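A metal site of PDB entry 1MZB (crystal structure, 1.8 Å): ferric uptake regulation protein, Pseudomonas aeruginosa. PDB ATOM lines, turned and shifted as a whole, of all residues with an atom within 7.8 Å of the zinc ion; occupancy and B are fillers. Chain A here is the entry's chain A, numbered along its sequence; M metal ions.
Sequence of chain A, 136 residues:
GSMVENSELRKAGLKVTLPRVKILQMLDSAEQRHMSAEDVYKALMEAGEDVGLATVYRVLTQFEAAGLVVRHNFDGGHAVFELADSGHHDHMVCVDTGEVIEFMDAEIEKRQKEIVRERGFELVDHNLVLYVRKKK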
ATOM      1  N   ARG A  33      21.527  -9.492 -15.304  1.00  0.00           N
ATOM      2  CA  ARG A  33      22.010  -8.210 -14.818  1.00  0.00           C
ATOM      3  C   ARG A  33      20.881  -7.170 -14.802  1.00  0.00           C
ATOM      4  O   ARG A  33      20.841  -6.281 -13.919  1.00  0.00           O
ATOM      5  CB  ARG A  33      23.163  -7.717 -15.703  1.00  0.00           C
ATOM      6  CG  ARG A  33      24.164  -8.802 -16.110  1.00  0.00           C
ATOM      7  CD  ARG A  33      25.461  -8.165 -16.616  1.00  0.00           C
ATOM      8  NE  ARG A  33      26.376  -9.140 -17.204  1.00  0.00           N
ATOM      9  CZ  ARG A  33      27.632  -8.857 -17.539  1.00  0.00           C
ATOM     10  NH1 ARG A  33      28.111  -7.629 -17.347  1.00  0.00           N
ATOM     11  NH2 ARG A  33      28.414  -9.798 -18.083  1.00  0.00           N
ATOM     12  N   HIS A  34      19.962  -7.311 -15.760  1.00  0.00           N
ATOM     13  CA  HIS A  34      18.824  -6.399 -15.925  1.00  0.00           C
ATOM     14  C   HIS A  34      17.479  -7.109 -15.774  1.00  0.00           C
ATOM     15  O   HIS A  34      16.829  -7.504 -16.742  1.00  0.00           O
ATOM     16  CB  HIS A  34      18.901  -5.720 -17.283  1.00  0.00           C
ATOM     17  CG  HIS A  34      20.236  -5.112 -17.557  1.00  0.00           C
ATOM     18  ND1 HIS A  34      21.215  -5.792 -18.249  1.00  0.00           N
ATOM     19  CD2 HIS A  34      20.735  -3.925 -17.136  1.00  0.00           C
ATOM     20  CE1 HIS A  34      22.286  -5.021 -18.222  1.00  0.00           C
ATOM     21  NE2 HIS A  34      22.050  -3.869 -17.562  1.00  0.00           N
ATOM     22  N   HIS A  72      15.130   1.356 -16.058  1.00  0.00           N
ATOM     23  CA  HIS A  72      15.403   1.601 -17.458  1.00  0.00           C
ATOM     24  C   HIS A  72      14.305   0.884 -18.276  1.00  0.00           C
ATOM     25  O   HIS A  72      13.700  -0.054 -17.787  1.00  0.00           O
ATOM     26  CB  HIS A  72      16.725   0.941 -17.884  1.00  0.00           C
ATOM     27  CG  HIS A  72      17.957   1.667 -17.425  1.00  0.00           C
ATOM     28  ND1 HIS A  72      18.843   1.108 -16.521  1.00  0.00           N
ATOM     29  CD2 HIS A  72      18.520   2.815 -17.850  1.00  0.00           C
ATOM     30  CE1 HIS A  72      19.902   1.893 -16.410  1.00  0.00           C
ATOM     31  NE2 HIS A  72      19.738   2.933 -17.215  1.00  0.00           N
ATOM     32  N   PHE A  74      14.436  -0.536 -21.923  1.00  0.00           N
ATOM     33  CA  PHE A  74      15.241  -0.675 -23.142  1.00  0.00           C
ATOM     34  C   PHE A  74      14.511  -1.147 -24.390  1.00  0.00           C
ATOM     35  O   PHE A  74      14.902  -0.758 -25.506  1.00  0.00           O
ATOM     36  CB  PHE A  74      16.404  -1.645 -22.896  1.00  0.00           C
ATOM     37  CG  PHE A  74      17.355  -1.202 -21.798  1.00  0.00           C
ATOM     38  CD1 PHE A  74      18.025   0.019 -21.885  1.00  0.00           C
ATOM     39  CD2 PHE A  74      17.633  -2.061 -20.729  1.00  0.00           C
ATOM     40  CE1 PHE A  74      19.005   0.375 -20.912  1.00  0.00           C
ATOM     41  CE2 PHE A  74      18.581  -1.705 -19.755  1.00  0.00           C
ATOM     42  CZ  PHE A  74      19.264  -0.495 -19.845  1.00  0.00           C
ATOM     43  N   VAL A  80      13.239  -2.445 -16.527  1.00  0.00           N
ATOM     44  CA  VAL A  80      14.321  -3.241 -16.001  1.00  0.00           C
ATOM     45  C   VAL A  80      14.798  -2.504 -14.755  1.00  0.00           C
ATOM     46  O   VAL A  80      14.866  -1.284 -14.794  1.00  0.00           O
ATOM     47  CB  VAL A  80      15.478  -3.275 -17.008  1.00  0.00           C
ATOM     48  CG1 VAL A  80      16.805  -3.522 -16.325  1.00  0.00           C
ATOM     49  CG2 VAL A  80      15.173  -4.366 -18.040  1.00  0.00           C
ATOM     50  N   PHE A  81      15.151  -3.224 -13.684  1.00  0.00           N
ATOM     51  CA  PHE A  81      15.619  -2.544 -12.480  1.00  0.00           C
ATOM     52  C   PHE A  81      17.005  -3.093 -12.190  1.00  0.00           C
ATOM     53  O   PHE A  81      17.196  -4.295 -12.237  1.00  0.00           O
ATOM     54  CB  PHE A  81      14.713  -2.867 -11.288  1.00  0.00           C
ATOM     55  CG  PHE A  81      13.315  -2.310 -11.421  1.00  0.00           C
ATOM     56  CD1 PHE A  81      12.319  -3.015 -12.091  1.00  0.00           C
ATOM     57  CD2 PHE A  81      12.991  -1.069 -10.854  1.00  0.00           C
ATOM     58  CE1 PHE A  81      10.982  -2.490 -12.183  1.00  0.00           C
ATOM     59  CE2 PHE A  81      11.686  -0.545 -10.946  1.00  0.00           C
ATOM     60  CZ  PHE A  81      10.674  -1.261 -11.605  1.00  0.00           C
ATOM     61  N   GLU A  82      17.976  -2.227 -11.944  1.00  0.00           N
ATOM     62  CA  GLU A  82      19.327  -2.725 -11.659  1.00  0.00           C
ATOM     63  C   GLU A  82      19.906  -1.869 -10.558  1.00  0.00           C
ATOM     64  O   GLU A  82      19.485  -0.747 -10.368  1.00  0.00           O
ATOM     65  CB  GLU A  82      20.211  -2.686 -12.899  1.00  0.00           C
ATOM     66  CG  GLU A  82      20.333  -1.310 -13.582  1.00  0.00           C
ATOM     67  CD  GLU A  82      21.050  -1.379 -14.945  1.00  0.00           C
ATOM     68  OE1 GLU A  82      22.260  -1.653 -14.986  1.00  0.00           O
ATOM     69  OE2 GLU A  82      20.388  -1.155 -15.972  1.00  0.00           O
ATOM     70  N   LEU A  83      20.828  -2.425  -9.795  1.00  0.00           N
ATOM     71  CA  LEU A  83      21.424  -1.643  -8.736  1.00  0.00           C
ATOM     72  C   LEU A  83      22.112  -0.402  -9.283  1.00  0.00           C
ATOM     73  O   LEU A  83      22.570  -0.357 -10.449  1.00  0.00           O
ATOM     74  CB  LEU A  83      22.426  -2.515  -7.984  1.00  0.00           C
ATOM     75  CG  LEU A  83      21.786  -3.691  -7.281  1.00  0.00           C
ATOM     76  CD1 LEU A  83      22.908  -4.602  -6.745  1.00  0.00           C
ATOM     77  CD2 LEU A  83      20.869  -3.188  -6.124  1.00  0.00           C
ATOM     78  N   SER A  86      26.498  -0.446  -8.118  1.00  0.00           N
ATOM     79  CA  SER A  86      27.479  -1.100  -8.972  1.00  0.00           C
ATOM     80  C   SER A  86      28.275  -0.066  -9.769  1.00  0.00           C
ATOM     81  O   SER A  86      27.850   1.092  -9.915  1.00  0.00           O
ATOM     82  CB  SER A  86      26.780  -2.063  -9.938  1.00  0.00           C
ATOM     83  OG  SER A  86      25.891  -1.355 -10.803  1.00  0.00           O
ATOM     84  N   GLY A  87      29.434  -0.471 -10.303  1.00  0.00           N
ATOM     85  CA  GLY A  87      30.225   0.447 -11.100  1.00  0.00           C
ATOM     86  C   GLY A  87      29.302   1.036 -12.155  1.00  0.00           C
ATOM     87  O   GLY A  87      28.312   0.408 -12.540  1.00  0.00           O
ATOM     88  N   HIS A  88      29.607   2.241 -12.618  1.00  0.00           N
ATOM     89  CA  HIS A  88      28.769   2.882 -13.630  1.00  0.00           C
ATOM     90  C   HIS A  88      28.842   2.145 -14.961  1.00  0.00           C
ATOM     91  O   HIS A  88      29.883   1.573 -15.331  1.00  0.00           O
ATOM     92  CB  HIS A  88      29.198   4.336 -13.855  1.00  0.00           C
ATOM     93  CG  HIS A  88      28.597   4.984 -15.078  1.00  0.00           C
ATOM     94  ND1 HIS A  88      27.273   5.343 -15.152  1.00  0.00           N
ATOM     95  CD2 HIS A  88      29.167   5.378 -16.236  1.00  0.00           C
ATOM     96  CE1 HIS A  88      27.051   5.952 -16.304  1.00  0.00           C
ATOM     97  NE2 HIS A  88      28.193   5.988 -16.991  1.00  0.00           N
ATOM     98  N   HIS A  89      27.720   2.162 -15.672  1.00  0.00           N
ATOM     99  CA  HIS A  89      27.613   1.514 -16.967  1.00  0.00           C
ATOM    100  C   HIS A  89      26.507   2.165 -17.781  1.00  0.00           C
ATOM    101  O   HIS A  89      25.451   2.520 -17.261  1.00  0.00           O
ATOM    102  CB  HIS A  89      27.333   0.014 -16.777  1.00  0.00           C
ATOM    103  N   ASP A  90      26.778   2.373 -19.064  1.00  0.00           N
ATOM    104  CA  ASP A  90      25.772   2.919 -19.950  1.00  0.00           C
ATOM    105  C   ASP A  90      25.400   1.674 -20.736  1.00  0.00           C
ATOM    106  O   ASP A  90      25.891   0.613 -20.424  1.00  0.00           O
ATOM    107  CB  ASP A  90      26.376   3.974 -20.811  1.00  0.00           C
ATOM    108  CG  ASP A  90      26.914   5.134 -19.953  1.00  0.00           C
ATOM    109  OD1 ASP A  90      26.162   5.650 -19.120  1.00  0.00           O
ATOM    110  OD2 ASP A  90      28.034   5.488 -20.141  1.00  0.00           O
ATOM    111  N   HIS A  91      24.558   1.778 -21.751  1.00  0.00           N
ATOM    112  CA  HIS A  91      24.125   0.540 -22.404  1.00  0.00           C
ATOM    113  C   HIS A  91      24.002   0.591 -23.902  1.00  0.00           C
ATOM    114  O   HIS A  91      23.602   1.621 -24.452  1.00  0.00           O
ATOM    115  CB  HIS A  91      22.721   0.124 -21.868  1.00  0.00           C
ATOM    116  CG  HIS A  91      22.640  -0.064 -20.380  1.00  0.00           C
ATOM    117  ND1 HIS A  91      22.544   1.003 -19.510  1.00  0.00           N
ATOM    118  CD2 HIS A  91      22.684  -1.209 -19.675  1.00  0.00           C
ATOM    119  CE1 HIS A  91      22.538   0.474 -18.310  1.00  0.00           C
ATOM    120  NE2 HIS A  91      22.627  -0.837 -18.358  1.00  0.00           N
ATOM    121  N   VAL A 100      20.909  -6.541 -24.249  1.00  0.00           N
ATOM    122  CA  VAL A 100      21.489  -5.334 -23.630  1.00  0.00           C
ATOM    123  C   VAL A 100      22.930  -5.613 -23.294  1.00  0.00           C
ATOM    124  O   VAL A 100      23.253  -6.632 -22.627  1.00  0.00           O
ATOM    125  CB  VAL A 100      20.734  -4.972 -22.349  1.00  0.00           C
ATOM    126  CG1 VAL A 100      21.370  -3.757 -21.672  1.00  0.00           C
ATOM    127  CG2 VAL A 100      19.251  -4.678 -22.710  1.00  0.00           C
ATOM    128  N   ILE A 101      23.791  -4.698 -23.722  1.00  0.00           N
ATOM    129  CA  ILE A 101      25.238  -4.800 -23.526  1.00  0.00           C
ATOM    130  C   ILE A 101      25.708  -3.570 -22.744  1.00  0.00           C
ATOM    131  O   ILE A 101      25.576  -2.438 -23.198  1.00  0.00           O
ATOM    132  CB  ILE A 101      25.952  -4.831 -24.910  1.00  0.00           C
ATOM    133  CG1 ILE A 101      25.475  -6.047 -25.704  1.00  0.00           C
ATOM    134  CG2 ILE A 101      27.485  -4.819 -24.729  1.00  0.00           C
ATOM    135  CD1 ILE A 101      25.800  -5.975 -27.179  1.00  0.00           C
ATOM    136  N   GLU A 102      26.247  -3.795 -21.544  1.00  0.00           N
ATOM    137  CA  GLU A 102      26.772  -2.669 -20.763  1.00  0.00           C
ATOM    138  C   GLU A 102      28.161  -2.251 -21.273  1.00  0.00           C
ATOM    139  O   GLU A 102      28.949  -3.078 -21.774  1.00  0.00           O
ATOM    140  CB  GLU A 102      26.910  -3.027 -19.278  1.00  0.00           C
ATOM    141  CG  GLU A 102      25.592  -3.148 -18.529  1.00  0.00           C
ATOM    142  CD  GLU A 102      25.781  -3.244 -17.020  1.00  0.00           C
ATOM    143  OE1 GLU A 102      26.867  -3.707 -16.588  1.00  0.00           O
ATOM    144  OE2 GLU A 102      24.842  -2.893 -16.268  1.00  0.00           O
ATOM    145  N   PHE A 103      28.467  -0.961 -21.157  1.00  0.00           N
ATOM    146  CA  PHE A 103      29.791  -0.458 -21.524  1.00  0.00           C
ATOM    147  C   PHE A 103      30.054   0.768 -20.686  1.00  0.00           C
ATOM    148  O   PHE A 103      29.140   1.337 -20.086  1.00  0.00           O
ATOM    149  CB  PHE A 103      29.893  -0.135 -23.017  1.00  0.00           C
ATOM    150  CG  PHE A 103      29.150   1.111 -23.434  1.00  0.00           C
ATOM    151  CD1 PHE A 103      27.797   1.067 -23.760  1.00  0.00           C
ATOM    152  CD2 PHE A 103      29.817   2.316 -23.506  1.00  0.00           C
ATOM    153  CE1 PHE A 103      27.110   2.222 -24.164  1.00  0.00           C
ATOM    154  CE2 PHE A 103      29.160   3.492 -23.904  1.00  0.00           C
ATOM    155  CZ  PHE A 103      27.797   3.439 -24.234  1.00  0.00           C
HETATM  156 ZN    ZN M   1      22.886  -2.193 -16.848  1.00  0.00          ZN
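Of the 18 residues printed, 4 come within 4 Å of the zinc ion.
A ring nitrogen (NE2) of His 34 is bound to the zinc ion. OE1 of Glu 82 binds the zinc ion, 2.0 Å away. NE2 of His 91 binds the zinc ion, 2.0 Å away. The zinc ion is bound by OE2 of Glu 102 (2.2 Å). Slightly farther from the zinc ion lies OE2 of Glu 82 (2.8 Å).
OE2 of Glu 82 is in hydrogen-bond range of ND1 of His 72 (2.8 Å).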
